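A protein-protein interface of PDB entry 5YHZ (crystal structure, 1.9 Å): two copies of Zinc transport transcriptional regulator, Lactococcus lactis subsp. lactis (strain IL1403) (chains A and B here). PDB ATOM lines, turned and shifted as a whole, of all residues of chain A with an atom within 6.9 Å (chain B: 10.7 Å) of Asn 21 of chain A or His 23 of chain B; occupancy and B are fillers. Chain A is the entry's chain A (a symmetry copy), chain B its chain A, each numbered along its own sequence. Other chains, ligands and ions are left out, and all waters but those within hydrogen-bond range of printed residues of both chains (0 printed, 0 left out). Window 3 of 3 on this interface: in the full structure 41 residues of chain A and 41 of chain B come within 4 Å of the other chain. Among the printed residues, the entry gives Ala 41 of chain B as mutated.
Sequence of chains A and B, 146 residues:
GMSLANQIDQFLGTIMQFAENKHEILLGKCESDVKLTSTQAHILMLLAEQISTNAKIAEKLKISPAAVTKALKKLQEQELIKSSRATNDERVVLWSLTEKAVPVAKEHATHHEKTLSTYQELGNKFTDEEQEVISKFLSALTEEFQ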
ATOM      1  N   LEU A  12      -5.442 -23.789 -22.140  1.00  0.00           N
ATOM      2  CA  LEU A  12      -6.115 -24.903 -21.434  1.00  0.00           C
ATOM      3  C   LEU A  12      -7.650 -24.777 -21.518  1.00  0.00           C
ATOM      4  O   LEU A  12      -8.379 -25.799 -21.539  1.00  0.00           O
ATOM      5  CB  LEU A  12      -5.694 -24.918 -19.974  1.00  0.00           C
ATOM      6  CG  LEU A  12      -4.201 -25.279 -19.828  1.00  0.00           C
ATOM      7  CD1 LEU A  12      -3.756 -25.083 -18.400  1.00  0.00           C
ATOM      8  CD2 LEU A  12      -3.962 -26.736 -20.325  1.00  0.00           C
ATOM      9  N   GLY A  13      -8.147 -23.543 -21.556  1.00  0.00           N
ATOM     10  CA  GLY A  13      -9.584 -23.314 -21.678  1.00  0.00           C
ATOM     11  C   GLY A  13     -10.056 -23.824 -23.035  1.00  0.00           C
ATOM     12  O   GLY A  13     -11.172 -24.360 -23.193  1.00  0.00           O
ATOM     13  N   MET A  16     -10.350 -27.649 -22.915  1.00  0.00           N
ATOM     14  CA  MET A  16     -11.597 -28.056 -22.217  1.00  0.00           C
ATOM     15  C   MET A  16     -12.834 -27.789 -23.079  1.00  0.00           C
ATOM     16  O   MET A  16     -13.732 -28.623 -23.158  1.00  0.00           O
ATOM     17  CB  MET A  16     -11.687 -27.280 -20.914  1.00  0.00           C
ATOM     18  CG  MET A  16     -10.525 -27.672 -19.982  1.00  0.00           C
ATOM     19  SD  MET A  16     -10.208 -29.487 -19.929  1.00  0.00           S
ATOM     20  CE  MET A  16     -11.813 -29.770 -19.200  1.00  0.00           C
ATOM     21  N   GLN A  17     -12.880 -26.638 -23.744  1.00  0.00           N
ATOM     22  CA  GLN A  17     -13.925 -26.361 -24.751  1.00  0.00           C
ATOM     23  C   GLN A  17     -13.903 -27.427 -25.846  1.00  0.00           C
ATOM     24  O   GLN A  17     -14.925 -27.974 -26.242  1.00  0.00           O
ATOM     25  CB  GLN A  17     -13.656 -24.987 -25.368  1.00  0.00           C
ATOM     26  CG  GLN A  17     -14.851 -24.164 -25.825  1.00  0.00           C
ATOM     27  CD  GLN A  17     -14.607 -22.650 -25.653  1.00  0.00           C
ATOM     28  OE1 GLN A  17     -13.501 -22.224 -25.315  1.00  0.00           O
ATOM     29  NE2 GLN A  17     -15.655 -21.846 -25.854  1.00  0.00           N
ATOM     30  N   PHE A  18     -12.723 -27.779 -26.313  1.00  0.00           N
ATOM     31  CA  PHE A  18     -12.631 -28.690 -27.431  1.00  0.00           C
ATOM     32  C   PHE A  18     -13.003 -30.118 -27.011  1.00  0.00           C
ATOM     33  O   PHE A  18     -13.613 -30.859 -27.774  1.00  0.00           O
ATOM     34  CB  PHE A  18     -11.224 -28.649 -28.009  1.00  0.00           C
ATOM     35  CG  PHE A  18     -11.007 -29.605 -29.132  1.00  0.00           C
ATOM     36  CD1 PHE A  18     -10.633 -30.912 -28.876  1.00  0.00           C
ATOM     37  CD2 PHE A  18     -11.193 -29.198 -30.446  1.00  0.00           C
ATOM     38  CE1 PHE A  18     -10.433 -31.808 -29.912  1.00  0.00           C
ATOM     39  CE2 PHE A  18     -10.993 -30.085 -31.491  1.00  0.00           C
ATOM     40  CZ  PHE A  18     -10.622 -31.392 -31.224  1.00  0.00           C
ATOM     41  N   ALA A  19     -12.655 -30.471 -25.781  1.00  0.00           N
ATOM     42  CA  ALA A  19     -12.889 -31.801 -25.259  1.00  0.00           C
ATOM     43  C   ALA A  19     -14.383 -31.997 -25.065  1.00  0.00           C
ATOM     44  O   ALA A  19     -14.888 -33.104 -25.245  1.00  0.00           O
ATOM     45  CB  ALA A  19     -12.185 -31.997 -23.900  1.00  0.00           C
ATOM     46  N   GLU A  20     -15.083 -30.916 -24.704  1.00  0.00           N
ATOM     47  CA  GLU A  20     -16.488 -30.994 -24.321  1.00  0.00           C
ATOM     48  C   GLU A  20     -16.662 -32.115 -23.307  1.00  0.00           C
ATOM     49  O   GLU A  20     -16.067 -32.045 -22.227  1.00  0.00           O
ATOM     50  CB  GLU A  20     -17.385 -31.172 -25.546  1.00  0.00           C
ATOM     51  CG  GLU A  20     -17.653 -29.846 -26.241  1.00  0.00           C
ATOM     52  CD  GLU A  20     -18.465 -29.988 -27.514  1.00  0.00           C
ATOM     53  OE1 GLU A  20     -19.440 -30.762 -27.532  1.00  0.00           O
ATOM     54  OE2 GLU A  20     -18.113 -29.318 -28.508  1.00  0.00           O
ATOM     55  N   ASN A  21     -17.411 -33.160 -23.653  1.00  0.00           N
ATOM     56  CA  ASN A  21     -17.670 -34.238 -22.690  1.00  0.00           C
ATOM     57  C   ASN A  21     -16.736 -35.459 -22.797  1.00  0.00           C
ATOM     58  O   ASN A  21     -16.893 -36.436 -22.049  1.00  0.00           O
ATOM     59  CB  ASN A  21     -19.137 -34.678 -22.781  1.00  0.00           C
ATOM     60  CG  ASN A  21     -20.101 -33.550 -22.407  1.00  0.00           C
ATOM     61  OD1 ASN A  21     -20.973 -33.176 -23.197  1.00  0.00           O
ATOM     62  ND2 ASN A  21     -19.929 -32.986 -21.203  1.00  0.00           N
ATOM     63  N   LYS A  22     -15.777 -35.383 -23.729  1.00  0.00           N
ATOM     64  CA  LYS A  22     -14.798 -36.442 -24.000  1.00  0.00           C
ATOM     65  C   LYS A  22     -13.648 -36.360 -22.988  1.00  0.00           C
ATOM     66  O   LYS A  22     -13.473 -35.352 -22.343  1.00  0.00           O
ATOM     67  CB  LYS A  22     -14.228 -36.290 -25.421  1.00  0.00           C
ATOM     68  CG  LYS A  22     -15.271 -36.036 -26.548  1.00  0.00           C
ATOM     69  CD  LYS A  22     -16.381 -37.087 -26.588  1.00  0.00           C
ATOM     70  CE  LYS A  22     -17.158 -37.089 -27.922  1.00  0.00           C
ATOM     71  NZ  LYS A  22     -16.471 -37.807 -29.082  1.00  0.00           N
ATOM     72  N   HIS A  23     -12.858 -37.409 -22.855  1.00  0.00           N
ATOM     73  CA  HIS A  23     -11.802 -37.403 -21.869  1.00  0.00           C
ATOM     74  C   HIS A  23     -10.514 -37.669 -22.597  1.00  0.00           C
ATOM     75  O   HIS A  23      -9.510 -38.025 -21.984  1.00  0.00           O
ATOM     76  CB  HIS A  23     -12.062 -38.467 -20.792  1.00  0.00           C
ATOM     77  CG  HIS A  23     -13.297 -38.197 -20.003  1.00  0.00           C
ATOM     78  ND1 HIS A  23     -13.411 -37.121 -19.145  1.00  0.00           N
ATOM     79  CD2 HIS A  23     -14.487 -38.842 -19.962  1.00  0.00           C
ATOM     80  CE1 HIS A  23     -14.612 -37.133 -18.589  1.00  0.00           C
ATOM     81  NE2 HIS A  23     -15.286 -38.163 -19.073  1.00  0.00           N
ATOM     82  N   GLU A  24     -10.587 -37.535 -23.924  1.00  0.00           N
ATOM     83  CA  GLU A  24      -9.445 -37.792 -24.789  1.00  0.00           C
ATOM     84  C   GLU A  24      -9.407 -36.686 -25.824  1.00  0.00           C
ATOM     85  O   GLU A  24     -10.448 -36.374 -26.448  1.00  0.00           O
ATOM     86  CB  GLU A  24      -9.559 -39.154 -25.504  1.00  0.00           C
ATOM     87  CG  GLU A  24      -8.203 -39.591 -26.000  1.00  0.00           C
ATOM     88  CD  GLU A  24      -8.196 -40.784 -26.932  1.00  0.00           C
ATOM     89  OE1 GLU A  24      -7.184 -40.885 -27.629  1.00  0.00           O
ATOM     90  OE2 GLU A  24      -9.121 -41.626 -26.953  1.00  0.00           O
ATOM     91  N   ILE B  15      -3.937 -33.408 -18.614  1.00  0.00           N
ATOM     92  CA  ILE B  15      -4.928 -32.354 -18.408  1.00  0.00           C
ATOM     93  C   ILE B  15      -6.333 -33.003 -18.297  1.00  0.00           C
ATOM     94  O   ILE B  15      -7.096 -32.712 -17.397  1.00  0.00           O
ATOM     95  CB  ILE B  15      -4.916 -31.331 -19.615  1.00  0.00           C
ATOM     96  CG1 ILE B  15      -3.603 -30.513 -19.647  1.00  0.00           C
ATOM     97  CG2 ILE B  15      -6.125 -30.390 -19.509  1.00  0.00           C
ATOM     98  CD1 ILE B  15      -3.321 -29.833 -18.327  1.00  0.00           C
ATOM     99  N   MET B  16      -6.671 -33.866 -19.252  1.00  0.00           N
ATOM    100  CA  MET B  16      -7.983 -34.564 -19.256  1.00  0.00           C
ATOM    101  C   MET B  16      -8.155 -35.440 -18.012  1.00  0.00           C
ATOM    102  O   MET B  16      -9.220 -35.454 -17.400  1.00  0.00           O
ATOM    103  CB  MET B  16      -8.065 -35.414 -20.512  1.00  0.00           C
ATOM    104  CG  MET B  16      -8.053 -34.515 -21.762  1.00  0.00           C
ATOM    105  SD  MET B  16      -9.133 -33.030 -21.609  1.00  0.00           S
ATOM    106  CE  MET B  16     -10.584 -34.066 -21.509  1.00  0.00           C
ATOM    107  N   GLN B  17      -7.107 -36.158 -17.619  1.00  0.00           N
ATOM    108  CA  GLN B  17      -7.097 -36.882 -16.330  1.00  0.00           C
ATOM    109  C   GLN B  17      -7.344 -35.913 -15.174  1.00  0.00           C
ATOM    110  O   GLN B  17      -8.148 -36.155 -14.283  1.00  0.00           O
ATOM    111  CB  GLN B  17      -5.732 -37.550 -16.157  1.00  0.00           C
ATOM    112  CG  GLN B  17      -5.673 -38.864 -15.392  1.00  0.00           C
ATOM    113  CD  GLN B  17      -4.566 -39.794 -15.931  1.00  0.00           C
ATOM    114  OE1 GLN B  17      -3.769 -39.399 -16.784  1.00  0.00           O
ATOM    115  NE2 GLN B  17      -4.544 -41.041 -15.451  1.00  0.00           N
ATOM    116  N   PHE B  18      -6.691 -34.769 -15.205  1.00  0.00           N
ATOM    117  CA  PHE B  18      -6.780 -33.858 -14.088  1.00  0.00           C
ATOM    118  C   PHE B  18      -8.158 -33.186 -14.033  1.00  0.00           C
ATOM    119  O   PHE B  18      -8.696 -32.940 -12.959  1.00  0.00           O
ATOM    120  CB  PHE B  18      -5.677 -32.815 -14.191  1.00  0.00           C
ATOM    121  CG  PHE B  18      -5.722 -31.784 -13.115  1.00  0.00           C
ATOM    122  CD1 PHE B  18      -6.509 -30.655 -13.259  1.00  0.00           C
ATOM    123  CD2 PHE B  18      -4.986 -31.954 -11.949  1.00  0.00           C
ATOM    124  CE1 PHE B  18      -6.559 -29.695 -12.263  1.00  0.00           C
ATOM    125  CE2 PHE B  18      -5.027 -30.997 -10.948  1.00  0.00           C
ATOM    126  CZ  PHE B  18      -5.820 -29.873 -11.100  1.00  0.00           C
ATOM    127  N   ALA B  19      -8.725 -32.927 -15.203  1.00  0.00           N
ATOM    128  CA  ALA B  19      -9.999 -32.248 -15.317  1.00  0.00           C
ATOM    129  C   ALA B  19     -11.095 -33.170 -14.808  1.00  0.00           C
ATOM    130  O   ALA B  19     -12.073 -32.704 -14.226  1.00  0.00           O
ATOM    131  CB  ALA B  19     -10.305 -31.880 -16.784  1.00  0.00           C
ATOM    132  N   GLU B  20     -10.919 -34.478 -15.027  1.00  0.00           N
ATOM    133  CA  GLU B  20     -11.964 -35.458 -14.745  1.00  0.00           C
ATOM    134  C   GLU B  20     -13.270 -34.976 -15.358  1.00  0.00           C
ATOM    135  O   GLU B  20     -13.338 -34.818 -16.581  1.00  0.00           O
ATOM    136  CB  GLU B  20     -12.084 -35.720 -13.245  1.00  0.00           C
ATOM    137  CG  GLU B  20     -11.034 -36.707 -12.762  1.00  0.00           C
ATOM    138  CD  GLU B  20     -11.060 -36.928 -11.262  1.00  0.00           C
ATOM    139  OE1 GLU B  20     -12.155 -37.047 -10.682  1.00  0.00           O
ATOM    140  OE2 GLU B  20      -9.966 -36.974 -10.660  1.00  0.00           O
ATOM    141  N   ASN B  21     -14.277 -34.690 -14.536  1.00  0.00           N
ATOM    142  CA  ASN B  21     -15.583 -34.288 -15.074  1.00  0.00           C
ATOM    143  C   ASN B  21     -15.825 -32.767 -15.155  1.00  0.00           C
ATOM    144  O   ASN B  21     -16.910 -32.326 -15.566  1.00  0.00           O
ATOM    145  CB  ASN B  21     -16.707 -34.967 -14.281  1.00  0.00           C
ATOM    146  CG  ASN B  21     -16.661 -36.491 -14.406  1.00  0.00           C
ATOM    147  OD1 ASN B  21     -16.576 -37.204 -13.402  1.00  0.00           O
ATOM    148  ND2 ASN B  21     -16.692 -36.994 -15.648  1.00  0.00           N
ATOM    149  N   LYS B  22     -14.809 -31.991 -14.758  1.00  0.00           N
ATOM    150  CA  LYS B  22     -14.844 -30.523 -14.744  1.00  0.00           C
ATOM    151  C   LYS B  22     -14.548 -29.981 -16.148  1.00  0.00           C
ATOM    152  O   LYS B  22     -14.031 -30.691 -16.980  1.00  0.00           O
ATOM    153  CB  LYS B  22     -13.793 -29.976 -13.763  1.00  0.00           C
ATOM    154  CG  LYS B  22     -13.746 -30.660 -12.365  1.00  0.00           C
ATOM    155  CD  LYS B  22     -15.102 -30.673 -11.657  1.00  0.00           C
ATOM    156  CE  LYS B  22     -14.984 -30.956 -10.144  1.00  0.00           C
ATOM    157  NZ  LYS B  22     -14.574 -29.765  -9.282  1.00  0.00           N
ATOM    158  N   HIS B  23     -14.860 -28.726 -16.411  1.00  0.00           N
ATOM    159  CA  HIS B  23     -14.660 -28.190 -17.737  1.00  0.00           C
ATOM    160  C   HIS B  23     -13.773 -26.984 -17.599  1.00  0.00           C
ATOM    161  O   HIS B  23     -13.691 -26.159 -18.506  1.00  0.00           O
ATOM    162  CB  HIS B  23     -16.006 -27.819 -18.379  1.00  0.00           C
ATOM    163  CG  HIS B  23     -16.886 -29.002 -18.594  1.00  0.00           C
ATOM    164  ND1 HIS B  23     -16.584 -29.997 -19.503  1.00  0.00           N
ATOM    165  CD2 HIS B  23     -18.045 -29.372 -17.998  1.00  0.00           C
ATOM    166  CE1 HIS B  23     -17.537 -30.915 -19.475  1.00  0.00           C
ATOM    167  NE2 HIS B  23     -18.431 -30.563 -18.566  1.00  0.00           N
ATOM    168  N   GLU B  24     -13.153 -26.881 -16.421  1.00  0.00           N
ATOM    169  CA  GLU B  24     -12.286 -25.758 -16.100  1.00  0.00           C
ATOM    170  C   GLU B  24     -11.060 -26.317 -15.408  1.00  0.00           C
ATOM    171  O   GLU B  24     -11.189 -27.134 -14.467  1.00  0.00           O
ATOM    172  CB  GLU B  24     -12.979 -24.744 -15.167  1.00  0.00           C
ATOM    173  CG  GLU B  24     -12.269 -23.414 -15.231  1.00  0.00           C
ATOM    174  CD  GLU B  24     -12.681 -22.396 -14.189  1.00  0.00           C
ATOM    175  OE1 GLU B  24     -11.856 -21.502 -13.990  1.00  0.00           O
ATOM    176  OE2 GLU B  24     -13.792 -22.433 -13.616  1.00  0.00           O
ATOM    177  N   ILE B  25      -9.878 -25.885 -15.842  1.00  0.00           N
ATOM    178  CA  ILE B  25      -8.669 -26.382 -15.231  1.00  0.00           C
ATOM    179  C   ILE B  25      -8.285 -25.437 -14.128  1.00  0.00           C
ATOM    180  O   ILE B  25      -7.943 -24.286 -14.359  1.00  0.00           O
ATOM    181  CB  ILE B  25      -7.500 -26.524 -16.229  1.00  0.00           C
ATOM    182  CG1 ILE B  25      -7.928 -27.322 -17.454  1.00  0.00           C
ATOM    183  CG2 ILE B  25      -6.306 -27.197 -15.505  1.00  0.00           C
ATOM    184  CD1 ILE B  25      -8.335 -28.735 -17.090  1.00  0.00           C
ATOM    185  N   LEU B  26      -8.284 -25.933 -12.910  1.00  0.00           N
ATOM    186  CA  LEU B  26      -8.008 -25.061 -11.795  1.00  0.00           C
ATOM    187  C   LEU B  26      -7.089 -25.776 -10.838  1.00  0.00           C
ATOM    188  O   LEU B  26      -7.335 -26.923 -10.523  1.00  0.00           O
ATOM    189  CB  LEU B  26      -9.353 -24.752 -11.083  1.00  0.00           C
ATOM    190  CG  LEU B  26     -10.234 -23.773 -11.828  1.00  0.00           C
ATOM    191  CD1 LEU B  26     -11.686 -23.686 -11.228  1.00  0.00           C
ATOM    192  CD2 LEU B  26      -9.598 -22.431 -11.741  1.00  0.00           C
ATOM    193  N   LYS B  35     -21.271 -28.195  -6.725  1.00  0.00           N
ATOM    194  CA  LYS B  35     -21.174 -28.453  -8.161  1.00  0.00           C
ATOM    195  C   LYS B  35     -21.634 -27.239  -8.951  1.00  0.00           C
ATOM    196  O   LYS B  35     -22.843 -26.951  -8.963  1.00  0.00           O
ATOM    197  CB  LYS B  35     -22.095 -29.624  -8.537  1.00  0.00           C
ATOM    198  CG  LYS B  35     -21.801 -30.930  -7.829  1.00  0.00           C
ATOM    199  CD  LYS B  35     -22.586 -32.081  -8.458  1.00  0.00           C
ATOM    200  CE  LYS B  35     -21.702 -33.303  -8.731  1.00  0.00           C
ATOM    201  NZ  LYS B  35     -22.105 -34.011  -9.986  1.00  0.00           N
ATOM    202  N   LEU B  36     -20.706 -26.541  -9.611  1.00  0.00           N
ATOM    203  CA  LEU B  36     -21.072 -25.362 -10.400  1.00  0.00           C
ATOM    204  C   LEU B  36     -20.498 -25.416 -11.783  1.00  0.00           C
ATOM    205  O   LEU B  36     -19.411 -25.941 -11.975  1.00  0.00           O
ATOM    206  CB  LEU B  36     -20.558 -24.077  -9.753  1.00  0.00           C
ATOM    207  CG  LEU B  36     -20.923 -23.752  -8.308  1.00  0.00           C
ATOM    208  CD1 LEU B  36     -20.158 -22.477  -7.915  1.00  0.00           C
ATOM    209  CD2 LEU B  36     -22.411 -23.561  -8.144  1.00  0.00           C
ATOM    210  N   THR B  37     -21.187 -24.847 -12.764  1.00  0.00           N
ATOM    211  CA  THR B  37     -20.531 -24.673 -14.028  1.00  0.00           C
ATOM    212  C   THR B  37     -19.508 -23.538 -13.852  1.00  0.00           C
ATOM    213  O   THR B  37     -19.494 -22.810 -12.842  1.00  0.00           O
ATOM    214  CB  THR B  37     -21.493 -24.323 -15.200  1.00  0.00           C
ATOM    215  OG1 THR B  37     -21.944 -22.974 -15.067  1.00  0.00           O
ATOM    216  CG2 THR B  37     -22.671 -25.253 -15.261  1.00  0.00           C
ATOM    217  N   SER B  38     -18.667 -23.361 -14.859  1.00  0.00           N
ATOM    218  CA  SER B  38     -17.676 -22.326 -14.784  1.00  0.00           C
ATOM    219  C   SER B  38     -18.368 -20.982 -14.904  1.00  0.00           C
ATOM    220  O   SER B  38     -17.955 -20.015 -14.248  1.00  0.00           O
ATOM    221  CB  SER B  38     -16.632 -22.512 -15.894  1.00  0.00           C
ATOM    222  OG  SER B  38     -17.277 -22.525 -17.161  1.00  0.00           O
ATOM    223  N   THR B  39     -19.373 -20.895 -15.784  1.00  0.00           N
ATOM    224  CA  THR B  39     -20.091 -19.623 -15.952  1.00  0.00           C
ATOM    225  C   THR B  39     -20.794 -19.248 -14.606  1.00  0.00           C
ATOM    226  O   THR B  39     -20.799 -18.117 -14.155  1.00  0.00           O
ATOM    227  CB  THR B  39     -21.175 -19.688 -17.072  1.00  0.00           C
ATOM    228  OG1 THR B  39     -20.647 -20.319 -18.254  1.00  0.00           O
ATOM    229  CG2 THR B  39     -21.682 -18.264 -17.390  1.00  0.00           C
ATOM    230  N   GLN B  40     -21.362 -20.237 -13.963  1.00  0.00           N
ATOM    231  CA  GLN B  40     -21.962 -19.994 -12.683  1.00  0.00           C
ATOM    232  C   GLN B  40     -20.949 -19.539 -11.650  1.00  0.00           C
ATOM    233  O   GLN B  40     -21.227 -18.594 -10.907  1.00  0.00           O
ATOM    234  CB  GLN B  40     -22.672 -21.259 -12.232  1.00  0.00           C
ATOM    235  CG  GLN B  40     -23.778 -21.635 -13.204  1.00  0.00           C
ATOM    236  CD  GLN B  40     -24.171 -23.039 -13.096  1.00  0.00           C
ATOM    237  OE1 GLN B  40     -23.889 -23.694 -12.090  1.00  0.00           O
ATOM    238  NE2 GLN B  40     -24.884 -23.529 -14.104  1.00  0.00           N
ATOM    239  N   ALA B  41     -19.759 -20.180 -11.598  1.00  0.00           N
ATOM    240  CA  ALA B  41     -18.780 -19.787 -10.582  1.00  0.00           C
ATOM    241  C   ALA B  41     -18.307 -18.389 -10.895  1.00  0.00           C
ATOM    242  O   ALA B  41     -18.003 -17.626 -10.007  1.00  0.00           O
ATOM    243  CB  ALA B  41     -17.547 -20.805 -10.507  1.00  0.00           C
ATOM    244  N   HIS B  42     -18.240 -18.004 -12.168  1.00  0.00           N
ATOM    245  CA  HIS B  42     -17.740 -16.697 -12.458  1.00  0.00           C
ATOM    246  C   HIS B  42     -18.752 -15.588 -12.133  1.00  0.00           C
ATOM    247  O   HIS B  42     -18.418 -14.495 -11.728  1.00  0.00           O
ATOM    248  CB  HIS B  42     -17.279 -16.664 -13.899  1.00  0.00           C
ATOM    249  CG  HIS B  42     -16.221 -17.684 -14.167  1.00  0.00           C
ATOM    250  ND1 HIS B  42     -15.810 -18.032 -15.435  1.00  0.00           N
ATOM    251  CD2 HIS B  42     -15.488 -18.438 -13.312  1.00  0.00           C
ATOM    252  CE1 HIS B  42     -14.872 -18.962 -15.353  1.00  0.00           C
ATOM    253  NE2 HIS B  42     -14.643 -19.215 -14.080  1.00  0.00           N
ATOM    254  N   HIS B 108     -13.392 -20.073  -5.399  1.00  0.00           N
ATOM    255  CA  HIS B 108     -13.184 -20.224  -6.829  1.00  0.00           C
ATOM    256  C   HIS B 108     -12.223 -19.159  -7.277  1.00  0.00           C
ATOM    257  O   HIS B 108     -11.262 -19.439  -8.009  1.00  0.00           O
ATOM    258  CB  HIS B 108     -14.506 -20.204  -7.585  1.00  0.00           C
ATOM    259  CG  HIS B 108     -14.403 -20.636  -9.013  1.00  0.00           C
ATOM    260  ND1 HIS B 108     -14.830 -21.872  -9.434  1.00  0.00           N
ATOM    261  CD2 HIS B 108     -13.926 -20.002 -10.111  1.00  0.00           C
ATOM    262  CE1 HIS B 108     -14.650 -21.978 -10.735  1.00  0.00           C
ATOM    263  NE2 HIS B 108     -14.104 -20.863 -11.166  1.00  0.00           N
ATOM    264  N   HIS B 112      -8.585 -19.360  -9.113  1.00  0.00           N
ATOM    265  CA  HIS B 112      -8.174 -18.620 -10.296  1.00  0.00           C
ATOM    266  C   HIS B 112      -6.800 -18.012  -9.971  1.00  0.00           C
ATOM    267  O   HIS B 112      -5.863 -18.079 -10.789  1.00  0.00           O
ATOM    268  CB  HIS B 112      -9.190 -17.512 -10.654  1.00  0.00           C
ATOM    269  CG  HIS B 112     -10.406 -17.987 -11.443  1.00  0.00           C
ATOM    270  ND1 HIS B 112     -11.052 -17.163 -12.335  1.00  0.00           N
ATOM    271  CD2 HIS B 112     -11.079 -19.162 -11.484  1.00  0.00           C
ATOM    272  CE1 HIS B 112     -12.060 -17.803 -12.905  1.00  0.00           C
ATOM    273  NE2 HIS B 112     -12.129 -19.004 -12.391  1.00  0.00           N
ATOM    274  N   TYR B 119       0.972 -20.347 -13.213  1.00  0.00           N
ATOM    275  CA  TYR B 119       1.405 -20.234 -14.585  1.00  0.00           C
ATOM    276  C   TYR B 119       2.368 -19.105 -14.763  1.00  0.00           C
ATOM    277  O   TYR B 119       3.339 -19.188 -15.554  1.00  0.00           O
ATOM    278  CB  TYR B 119       0.223 -19.954 -15.497  1.00  0.00           C
ATOM    279  CG  TYR B 119      -0.813 -21.072 -15.517  1.00  0.00           C
ATOM    280  CD1 TYR B 119      -0.500 -22.323 -15.058  1.00  0.00           C
ATOM    281  CD2 TYR B 119      -2.119 -20.812 -15.943  1.00  0.00           C
ATOM    282  CE1 TYR B 119      -1.450 -23.361 -15.082  1.00  0.00           C
ATOM    283  CE2 TYR B 119      -3.100 -21.795 -15.945  1.00  0.00           C
ATOM    284  CZ  TYR B 119      -2.769 -23.032 -15.542  1.00  0.00           C
ATOM    285  OH  TYR B 119      -3.720 -23.938 -15.588  1.00  0.00           O
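The backbone carbonyl oxygen of Glu 20 of chain B lies close to a ring nitrogen (ND1) of His 23 of chain A (3.4 Å).
ND1 of His 23 of chain B sits close to O of Glu 20 of chain A (3.4 Å).
Leu 12 of chain A touches Ile 15 of chain B.
CE of Met 16 of chain A touches CB of Ala 19 of chain B, at 3.5 Å.
Met 16 of chain A touches Lys 22 of chain B.
Met 16 of chain A touches His 23 of chain B (CB to O, 3.3 Å).
Met 16 of chain A touches Ile 25 of chain B (SD to CD1, 3.5 Å).
Ala 19 of chain A touches Met 16 of chain B.
ND2 of Asn 21 of chain A touches CE1 of His 23 of chain B, at 3.6 Å.
O of Lys 22 of chain A touches CE of Met 16 of chain B, 3.3 Å away.
Met 16 of chain B touches His 23 of chain A (CB to O, 3.3 Å).
CE1 of His 23 of chain A touches ND2 of Asn 21 of chain B, 3.6 Å away.
Asn 21 of chain A touches one residue of chain B.
His 23 of chain B touches just these residues of chain A: Met 16, Glu 20 and Asn 21.
Met 16 of chain A touches just these residues of chain B: Ala 19 (3.5 Å), Lys 22 (3.3 Å), His 23 (3.3 Å) and Ile 25 (3.5 Å).
Printed residues of chain B within 4 Å of Glu 20 of chain A: His 23.
Of the printed residues of chain B, Lys 22 of chain A touches Met 16 (3.3 Å).
Of the printed residues of chain A, Lys 22 of chain B touches Met 16.
Printed residues of chain A within 4 Å of Asn 21 of chain B: His 23.
Of the printed residues of chain B, Leu 12 of chain A touches Ile 15 (3.7 Å) and Tyr 119 (3.0 Å).
Phe 18 of chain A touches none of the printed residues of chain B.
The nearest residue of chain A that does not touch His 23 of chain B is Gln 17 of chain A (5.3 Å).
Printed residues of chain A that touch a printed residue of chain B: Leu 12, Met 16, Ala 19, Glu 20, Asn 21, Lys 22 and His 23.
Of the 23 printed residues of chain B, 9 touch a printed residue of chain A.
Among the printed residues, no Asp or Glu carboxylate lies within 4 Å of a Lys or Arg side-chain nitrogen of the other chain.
Met 16 of chain A touches Ala 19 of chain B, and with the chains exchanged Ala 19 of chain A touches Met 16 of chain B.
Met 16 of chain A touches Lys 22 of chain B, and with the chains exchanged Lys 22 of chain A touches Met 16 of chain B.
Glu 20 of chain A touches His 23 of chain B, and with the chains exchanged His 23 of chain A touches Glu 20 of chain B.
Asn 21 of chain A touches His 23 of chain B, and with the chains exchanged His 23 of chain A touches Asn 21 of chain B.
Positions printed for both chains: 16, 17, 18, 19, 20, 21, 22, 23 and 24.
Of the 13 pairs that touch across the chains among the printed residues, 10 have their exchanged pair printed and touching as well.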
